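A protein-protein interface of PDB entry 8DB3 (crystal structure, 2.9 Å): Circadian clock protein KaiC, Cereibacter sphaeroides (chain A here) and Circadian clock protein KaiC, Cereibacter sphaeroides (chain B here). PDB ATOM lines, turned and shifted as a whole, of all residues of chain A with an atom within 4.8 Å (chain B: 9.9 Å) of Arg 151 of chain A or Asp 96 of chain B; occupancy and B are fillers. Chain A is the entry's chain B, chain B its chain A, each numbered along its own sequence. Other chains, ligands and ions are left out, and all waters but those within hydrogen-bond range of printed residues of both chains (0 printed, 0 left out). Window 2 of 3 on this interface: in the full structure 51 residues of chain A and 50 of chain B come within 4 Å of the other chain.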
ATOM      1  N   LEU A 108       9.004  34.697 -20.552  1.00  0.00           N
ATOM      2  CA  LEU A 108       9.220  33.951 -19.317  1.00  0.00           C
ATOM      3  C   LEU A 108      10.667  34.062 -18.839  1.00  0.00           C
ATOM      4  O   LEU A 108      11.011  33.592 -17.752  1.00  0.00           O
ATOM      5  CB  LEU A 108       8.842  32.482 -19.513  1.00  0.00           C
ATOM      6  CG  LEU A 108       8.268  31.783 -18.279  1.00  0.00           C
ATOM      7  CD1 LEU A 108       6.897  32.350 -17.938  1.00  0.00           C
ATOM      8  CD2 LEU A 108       8.194  30.278 -18.491  1.00  0.00           C
ATOM      9  N   GLU A 109      11.515  34.681 -19.665  1.00  0.00           N
ATOM     10  CA  GLU A 109      12.882  34.962 -19.236  1.00  0.00           C
ATOM     11  C   GLU A 109      12.892  35.969 -18.092  1.00  0.00           C
ATOM     12  O   GLU A 109      13.702  35.859 -17.165  1.00  0.00           O
ATOM     13  CB  GLU A 109      13.707  35.479 -20.415  1.00  0.00           C
ATOM     14  N   PHE A 112      12.118  34.239 -14.912  1.00  0.00           N
ATOM     15  CA  PHE A 112      13.285  33.485 -14.465  1.00  0.00           C
ATOM     16  C   PHE A 112      14.277  34.391 -13.743  1.00  0.00           C
ATOM     17  O   PHE A 112      14.850  34.006 -12.716  1.00  0.00           O
ATOM     18  CB  PHE A 112      13.954  32.797 -15.657  1.00  0.00           C
ATOM     19  CG  PHE A 112      13.085  31.776 -16.351  1.00  0.00           C
ATOM     20  CD1 PHE A 112      11.946  31.272 -15.741  1.00  0.00           C
ATOM     21  CD2 PHE A 112      13.415  31.318 -17.616  1.00  0.00           C
ATOM     22  CE1 PHE A 112      11.156  30.337 -16.383  1.00  0.00           C
ATOM     23  CE2 PHE A 112      12.627  30.383 -18.262  1.00  0.00           C
ATOM     24  CZ  PHE A 112      11.499  29.891 -17.645  1.00  0.00           C
ATOM     25  N   ALA A 147       3.044  24.409 -22.651  1.00  0.00           N
ATOM     26  CA  ALA A 147       4.426  24.713 -22.997  1.00  0.00           C
ATOM     27  C   ALA A 147       5.055  25.629 -21.957  1.00  0.00           C
ATOM     28  O   ALA A 147       6.185  25.400 -21.515  1.00  0.00           O
ATOM     29  CB  ALA A 147       4.488  25.346 -24.387  1.00  0.00           C
ATOM     30  N   GLU A 148       4.330  26.673 -21.547  1.00  0.00           N
ATOM     31  CA  GLU A 148       4.883  27.600 -20.563  1.00  0.00           C
ATOM     32  C   GLU A 148       5.092  26.916 -19.216  1.00  0.00           C
ATOM     33  O   GLU A 148       6.123  27.120 -18.557  1.00  0.00           O
ATOM     34  CB  GLU A 148       3.968  28.815 -20.409  1.00  0.00           C
ATOM     35  CG  GLU A 148       3.725  29.580 -21.701  1.00  0.00           C
ATOM     36  CD  GLU A 148       4.722  30.703 -21.910  1.00  0.00           C
ATOM     37  OE1 GLU A 148       5.862  30.586 -21.414  1.00  0.00           O
ATOM     38  OE2 GLU A 148       4.364  31.699 -22.574  1.00  0.00           O
ATOM     39  N   ILE A 149       4.120  26.109 -18.784  1.00  0.00           N
ATOM     40  CA  ILE A 149       4.260  25.396 -17.520  1.00  0.00           C
ATOM     41  C   ILE A 149       5.501  24.517 -17.551  1.00  0.00           C
ATOM     42  O   ILE A 149       6.288  24.485 -16.596  1.00  0.00           O
ATOM     43  CB  ILE A 149       2.998  24.567 -17.225  1.00  0.00           C
ATOM     44  CG1 ILE A 149       1.833  25.487 -16.862  1.00  0.00           C
ATOM     45  CG2 ILE A 149       3.263  23.577 -16.099  1.00  0.00           C
ATOM     46  CD1 ILE A 149       0.485  24.809 -16.919  1.00  0.00           C
ATOM     47  N   ARG A 150       5.693  23.781 -18.649  1.00  0.00           N
ATOM     48  CA  ARG A 150       6.854  22.904 -18.730  1.00  0.00           C
ATOM     49  C   ARG A 150       8.145  23.712 -18.783  1.00  0.00           C
ATOM     50  O   ARG A 150       9.167  23.292 -18.232  1.00  0.00           O
ATOM     51  CB  ARG A 150       6.750  21.981 -19.947  1.00  0.00           C
ATOM     52  CG  ARG A 150       7.942  21.039 -20.088  1.00  0.00           C
ATOM     53  CD  ARG A 150       8.339  20.792 -21.543  1.00  0.00           C
ATOM     54  NE  ARG A 150       8.246  21.984 -22.375  1.00  0.00           N
ATOM     55  CZ  ARG A 150       8.531  22.022 -23.668  1.00  0.00           C
ATOM     56  NH1 ARG A 150       8.983  20.955 -24.306  1.00  0.00           N
ATOM     57  NH2 ARG A 150       8.356  23.156 -24.339  1.00  0.00           N
ATOM     58  N   ARG A 151       8.128  24.866 -19.452  1.00  0.00           N
ATOM     59  CA  ARG A 151       9.295  25.741 -19.432  1.00  0.00           C
ATOM     60  C   ARG A 151       9.682  26.079 -17.998  1.00  0.00           C
ATOM     61  O   ARG A 151      10.838  25.908 -17.588  1.00  0.00           O
ATOM     62  CB  ARG A 151       9.004  27.016 -20.226  1.00  0.00           C
ATOM     63  CG  ARG A 151       9.325  26.919 -21.710  1.00  0.00           C
ATOM     64  CD  ARG A 151      10.029  28.175 -22.210  1.00  0.00           C
ATOM     65  NE  ARG A 151       9.092  29.261 -22.473  1.00  0.00           N
ATOM     66  CZ  ARG A 151       9.432  30.538 -22.590  1.00  0.00           C
ATOM     67  NH1 ARG A 151      10.689  30.933 -22.470  1.00  0.00           N
ATOM     68  NH2 ARG A 151       8.487  31.441 -22.835  1.00  0.00           N
ATOM     69  N   LEU A 152       8.709  26.553 -17.216  1.00  0.00           N
ATOM     70  CA  LEU A 152       8.975  26.916 -15.826  1.00  0.00           C
ATOM     71  C   LEU A 152       9.476  25.720 -15.026  1.00  0.00           C
ATOM     72  O   LEU A 152      10.439  25.832 -14.254  1.00  0.00           O
ATOM     73  CB  LEU A 152       7.704  27.488 -15.198  1.00  0.00           C
ATOM     74  CG  LEU A 152       7.775  27.980 -13.754  1.00  0.00           C
ATOM     75  CD1 LEU A 152       9.081  28.701 -13.482  1.00  0.00           C
ATOM     76  CD2 LEU A 152       6.584  28.884 -13.455  1.00  0.00           C
ATOM     77  N   PHE A 153       8.842  24.561 -15.205  1.00  0.00           N
ATOM     78  CA  PHE A 153       9.192  23.407 -14.386  1.00  0.00           C
ATOM     79  C   PHE A 153      10.578  22.879 -14.741  1.00  0.00           C
ATOM     80  O   PHE A 153      11.337  22.470 -13.855  1.00  0.00           O
ATOM     81  CB  PHE A 153       8.136  22.314 -14.542  1.00  0.00           C
ATOM     82  CG  PHE A 153       6.869  22.576 -13.770  1.00  0.00           C
ATOM     83  CD1 PHE A 153       6.340  23.853 -13.689  1.00  0.00           C
ATOM     84  CD2 PHE A 153       6.208  21.541 -13.129  1.00  0.00           C
ATOM     85  CE1 PHE A 153       5.176  24.094 -12.981  1.00  0.00           C
ATOM     86  CE2 PHE A 153       5.043  21.777 -12.422  1.00  0.00           C
ATOM     87  CZ  PHE A 153       4.527  23.054 -12.348  1.00  0.00           C
ATOM     88  N   ASP A 154      10.937  22.897 -16.027  1.00  0.00           N
ATOM     89  CA  ASP A 154      12.272  22.467 -16.424  1.00  0.00           C
ATOM     90  C   ASP A 154      13.328  23.456 -15.943  1.00  0.00           C
ATOM     91  O   ASP A 154      14.426  23.054 -15.536  1.00  0.00           O
ATOM     92  CB  ASP A 154      12.340  22.300 -17.945  1.00  0.00           C
ATOM     93  CG  ASP A 154      11.357  21.260 -18.469  1.00  0.00           C
ATOM     94  OD1 ASP A 154      10.890  20.416 -17.674  1.00  0.00           O
ATOM     95  OD2 ASP A 154      11.053  21.288 -19.682  1.00  0.00           O
ATOM     96  N   TRP A 155      13.020  24.755 -15.983  1.00  0.00           N
ATOM     97  CA  TRP A 155      13.934  25.738 -15.412  1.00  0.00           C
ATOM     98  C   TRP A 155      14.193  25.435 -13.942  1.00  0.00           C
ATOM     99  O   TRP A 155      15.344  25.441 -13.480  1.00  0.00           O
ATOM    100  CB  TRP A 155      13.364  27.146 -15.584  1.00  0.00           C
ATOM    101  CG  TRP A 155      14.355  28.238 -15.297  1.00  0.00           C
ATOM    102  CD1 TRP A 155      15.296  28.740 -16.149  1.00  0.00           C
ATOM    103  CD2 TRP A 155      14.501  28.959 -14.069  1.00  0.00           C
ATOM    104  NE1 TRP A 155      16.018  29.729 -15.526  1.00  0.00           N
ATOM    105  CE2 TRP A 155      15.549  29.883 -14.249  1.00  0.00           C
ATOM    106  CE3 TRP A 155      13.846  28.914 -12.834  1.00  0.00           C
ATOM    107  CZ2 TRP A 155      15.957  30.753 -13.241  1.00  0.00           C
ATOM    108  CZ3 TRP A 155      14.253  29.777 -11.838  1.00  0.00           C
ATOM    109  CH2 TRP A 155      15.297  30.685 -12.046  1.00  0.00           C
ATOM    110  N   PHE B  61       7.889  14.127 -25.438  1.00  0.00           N
ATOM    111  CA  PHE B  61       7.619  15.463 -25.950  1.00  0.00           C
ATOM    112  C   PHE B  61       7.732  16.538 -24.883  1.00  0.00           C
ATOM    113  O   PHE B  61       7.649  17.727 -25.211  1.00  0.00           O
ATOM    114  CB  PHE B  61       6.215  15.514 -26.566  1.00  0.00           C
ATOM    115  CG  PHE B  61       6.095  14.764 -27.859  1.00  0.00           C
ATOM    116  CD1 PHE B  61       6.177  13.382 -27.884  1.00  0.00           C
ATOM    117  CD2 PHE B  61       5.900  15.441 -29.050  1.00  0.00           C
ATOM    118  CE1 PHE B  61       6.066  12.690 -29.072  1.00  0.00           C
ATOM    119  CE2 PHE B  61       5.788  14.754 -30.243  1.00  0.00           C
ATOM    120  CZ  PHE B  61       5.871  13.376 -30.254  1.00  0.00           C
ATOM    121  N   GLU B  62       7.935  16.157 -23.627  1.00  0.00           N
ATOM    122  CA  GLU B  62       7.857  17.106 -22.524  1.00  0.00           C
ATOM    123  C   GLU B  62       8.829  16.725 -21.419  1.00  0.00           C
ATOM    124  O   GLU B  62       9.639  17.552 -20.987  1.00  0.00           O
ATOM    125  CB  GLU B  62       6.421  17.156 -22.005  1.00  0.00           C
ATOM    126  CG  GLU B  62       6.274  17.695 -20.607  1.00  0.00           C
ATOM    127  CD  GLU B  62       4.859  18.144 -20.332  1.00  0.00           C
ATOM    128  OE1 GLU B  62       4.433  19.154 -20.932  1.00  0.00           O
ATOM    129  OE2 GLU B  62       4.167  17.474 -19.537  1.00  0.00           O
ATOM    130  N   GLU B  63       8.762  15.479 -20.963  1.00  0.00           N
ATOM    131  CA  GLU B  63       9.665  15.008 -19.924  1.00  0.00           C
ATOM    132  C   GLU B  63      11.094  14.922 -20.452  1.00  0.00           C
ATOM    133  O   GLU B  63      11.330  14.657 -21.633  1.00  0.00           O
ATOM    134  CB  GLU B  63       9.213  13.640 -19.410  1.00  0.00           C
ATOM    135  CG  GLU B  63       9.735  13.297 -18.023  1.00  0.00           C
ATOM    136  CD  GLU B  63       8.962  12.168 -17.359  1.00  0.00           C
ATOM    137  OE1 GLU B  63       7.986  11.666 -17.958  1.00  0.00           O
ATOM    138  OE2 GLU B  63       9.329  11.778 -16.228  1.00  0.00           O
ATOM    139  N   ARG B  64      12.055  15.143 -19.552  1.00  0.00           N
ATOM    140  CA  ARG B  64      13.462  15.149 -19.922  1.00  0.00           C
ATOM    141  C   ARG B  64      14.028  13.730 -19.932  1.00  0.00           C
ATOM    142  O   ARG B  64      13.588  12.872 -19.163  1.00  0.00           O
ATOM    143  CB  ARG B  64      14.258  16.017 -18.949  1.00  0.00           C
ATOM    144  CG  ARG B  64      14.171  17.510 -19.238  1.00  0.00           C
ATOM    145  CD  ARG B  64      14.010  18.331 -17.964  1.00  0.00           C
ATOM    146  NE  ARG B  64      14.717  17.741 -16.834  1.00  0.00           N
ATOM    147  CZ  ARG B  64      15.924  18.109 -16.422  1.00  0.00           C
ATOM    148  NH1 ARG B  64      16.593  19.080 -17.021  1.00  0.00           N
ATOM    149  NH2 ARG B  64      16.472  17.485 -15.385  1.00  0.00           N
ATOM    150  N   HIS B  92      14.066  13.669 -27.082  1.00  0.00           N
ATOM    151  CA  HIS B  92      13.293  14.760 -26.495  1.00  0.00           C
ATOM    152  C   HIS B  92      12.890  15.715 -27.611  1.00  0.00           C
ATOM    153  O   HIS B  92      13.743  16.354 -28.233  1.00  0.00           O
ATOM    154  CB  HIS B  92      14.104  15.479 -25.426  1.00  0.00           C
ATOM    155  CG  HIS B  92      13.376  16.617 -24.780  1.00  0.00           C
ATOM    156  ND1 HIS B  92      12.036  16.558 -24.463  1.00  0.00           N
ATOM    157  CD2 HIS B  92      13.800  17.841 -24.389  1.00  0.00           C
ATOM    158  CE1 HIS B  92      11.665  17.695 -23.905  1.00  0.00           C
ATOM    159  NE2 HIS B  92      12.717  18.492 -23.847  1.00  0.00           N
ATOM    160  N   ILE B  93      11.587  15.817 -27.854  1.00  0.00           N
ATOM    161  CA  ILE B  93      11.020  16.755 -28.816  1.00  0.00           C
ATOM    162  C   ILE B  93      10.297  17.830 -28.016  1.00  0.00           C
ATOM    163  O   ILE B  93       9.383  17.525 -27.240  1.00  0.00           O
ATOM    164  CB  ILE B  93      10.074  16.056 -29.802  1.00  0.00           C
ATOM    165  CG1 ILE B  93      10.710  14.766 -30.324  1.00  0.00           C
ATOM    166  CG2 ILE B  93       9.739  16.981 -30.959  1.00  0.00           C
ATOM    167  CD1 ILE B  93       9.804  13.952 -31.228  1.00  0.00           C
ATOM    168  N   ALA B  94      10.712  19.079 -28.188  1.00  0.00           N
ATOM    169  CA  ALA B  94      10.197  20.188 -27.400  1.00  0.00           C
ATOM    170  C   ALA B  94       9.419  21.152 -28.284  1.00  0.00           C
ATOM    171  O   ALA B  94       9.722  21.317 -29.469  1.00  0.00           O
ATOM    172  CB  ALA B  94      11.336  20.929 -26.693  1.00  0.00           C
ATOM    173  N   VAL B  95       8.412  21.792 -27.693  1.00  0.00           N
ATOM    174  CA  VAL B  95       7.529  22.703 -28.412  1.00  0.00           C
ATOM    175  C   VAL B  95       7.218  23.905 -27.528  1.00  0.00           C
ATOM    176  O   VAL B  95       7.006  23.766 -26.319  1.00  0.00           O
ATOM    177  CB  VAL B  95       6.228  21.997 -28.856  1.00  0.00           C
ATOM    178  CG1 VAL B  95       6.554  20.744 -29.665  1.00  0.00           C
ATOM    179  CG2 VAL B  95       5.359  21.651 -27.653  1.00  0.00           C
ATOM    180  N   ASP B  96       7.188  25.088 -28.140  1.00  0.00           N
ATOM    181  CA  ASP B  96       6.950  26.367 -27.480  1.00  0.00           C
ATOM    182  C   ASP B  96       6.246  27.257 -28.495  1.00  0.00           C
ATOM    183  O   ASP B  96       6.497  27.119 -29.698  1.00  0.00           O
ATOM    184  CB  ASP B  96       8.263  27.002 -27.001  1.00  0.00           C
ATOM    185  CG  ASP B  96       8.143  27.651 -25.626  1.00  0.00           C
ATOM    186  OD1 ASP B  96       7.322  27.196 -24.802  1.00  0.00           O
ATOM    187  OD2 ASP B  96       8.866  28.642 -25.382  1.00  0.00           O
ATOM    188  N   PRO B  97       5.412  28.226 -28.042  1.00  0.00           N
ATOM    189  CA  PRO B  97       4.369  28.790 -28.915  1.00  0.00           C
ATOM    190  C   PRO B  97       4.326  28.254 -30.335  1.00  0.00           C
ATOM    191  O   PRO B  97       4.850  28.872 -31.266  1.00  0.00           O
ATOM    192  CB  PRO B  97       4.701  30.291 -28.895  1.00  0.00           C
ATOM    193  CG  PRO B  97       5.209  30.515 -27.477  1.00  0.00           C
ATOM    194  CD  PRO B  97       5.736  29.162 -26.946  1.00  0.00           C
ATOM    195  N   SER B  98       3.690  27.100 -30.505  1.00  0.00           N
ATOM    196  CA  SER B  98       3.602  26.453 -31.809  1.00  0.00           C
ATOM    197  C   SER B  98       2.438  25.471 -31.837  1.00  0.00           C
ATOM    198  O   SER B  98       1.420  25.679 -31.173  1.00  0.00           O
ATOM    199  CB  SER B  98       4.910  25.736 -32.141  1.00  0.00           C
ATOM    200  OG  SER B  98       5.258  24.809 -31.128  1.00  0.00           O
ATOM    201  N   SER B 134       1.460  17.404 -25.867  1.00  0.00           N
ATOM    202  CA  SER B 134       2.184  18.634 -26.170  1.00  0.00           C
ATOM    203  C   SER B 134       1.819  19.159 -27.552  1.00  0.00           C
ATOM    204  O   SER B 134       1.678  20.372 -27.750  1.00  0.00           O
ATOM    205  CB  SER B 134       3.692  18.395 -26.088  1.00  0.00           C
ATOM    206  OG  SER B 134       4.052  17.806 -24.853  1.00  0.00           O
ATOM    207  N   LEU B 135       1.663  18.259 -28.519  1.00  0.00           N
ATOM    208  CA  LEU B 135       1.283  18.643 -29.872  1.00  0.00           C
ATOM    209  C   LEU B 135      -0.230  18.641 -30.055  1.00  0.00           C
ATOM    210  O   LEU B 135      -0.801  19.617 -30.551  1.00  0.00           O
ATOM    211  CB  LEU B 135       1.933  17.696 -30.885  1.00  0.00           C
ATOM    212  CG  LEU B 135       2.166  18.278 -32.279  1.00  0.00           C
ATOM    213  CD1 LEU B 135       3.480  17.760 -32.856  1.00  0.00           C
ATOM    214  CD2 LEU B 135       0.997  17.961 -33.204  1.00  0.00           C
ATOM    215  N   ALA B 138      -3.085  21.510 -29.305  1.00  0.00           N
ATOM    216  CA  ALA B 138      -3.245  22.719 -30.101  1.00  0.00           C
ATOM    217  C   ALA B 138      -4.276  22.567 -31.210  1.00  0.00           C
ATOM    218  O   ALA B 138      -4.698  23.575 -31.787  1.00  0.00           O
ATOM    219  CB  ALA B 138      -1.900  23.129 -30.712  1.00  0.00           C
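O of Phe 61 of chain B lies close to O of Ile 93 of chain B.
The guanidinium group of Arg 150 of chain A lies within salt-bridge range of the side-chain carboxylate of Asp 154 of chain A (3.95 Å).
The backbone carbonyl oxygen (O) of Asp 96 of chain B is in hydrogen-bond range of the side-chain hydroxyl (OG) of Ser 98 of chain B (3.0 Å).
The side-chain carboxylate of Glu 148 of chain A lies within salt-bridge range of the guanidinium group of Arg 151 of chain A (3.1 Å).
Of the 12 printed residues of chain A, 4 touch a printed residue of chain B.
Hydrophobic or aromatic side chains of chain A within 4 Å of the printed part of chain B: Ala 147.
Along chain A the printed residues that touch a printed residue of chain B span positions 147 to 154.
Among the printed residues, 8 pairs touch across the chains.
Among the printed residues, Asp or Glu carboxylates within 4 Å of a Lys or Arg side-chain nitrogen of the other chain: Arg 151 of chain A with Asp 96 of chain B (3.0 Å).
OD2 of Asp 96 of chain B is in salt-bridge range of NE of Arg 151 of chain A (3.0 Å).
O of Val 95 of chain B lies within hydrogen-bond range of NH2 of Arg 150 of chain A (2.5 Å).
Among the printed residues, merely in contact across the chains: Arg 150 of chain A with Ala 94 of chain B, Ala 147 of chain A with Asp 96 of chain B, Arg 150 of chain A with Glu 62 of chain B, Ala 147 of chain A with Val 95 of chain B, Arg 150 of chain A with Phe 61 of chain B and Asp 154 of chain A with Arg 64 of chain B.
Of the printed residues of chain B, Arg 151 of chain A touches Asp 96.
No residue of chain B comes within 4 Å of Leu 108 of chain A.
Of chain B, only Val 95 (3.5 Å) and Asp 96 (3.4 Å) come within 4 Å of Ala 147 of chain A.
Of the printed residues of chain A, Ala 94 of chain B touches Arg 150 (3.4 Å).
Of the printed residues of chain B, Arg 150 of chain A touches Phe 61, Glu 62, Ala 94 and Val 95.
The nearest residue of chain A that does not touch Asp 96 of chain B is Arg 150 of chain A (4.2 Å).
The nearest printed residue of chain A that does not touch Glu 62 of chain B is Asp 154 of chain A (4.2 Å).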
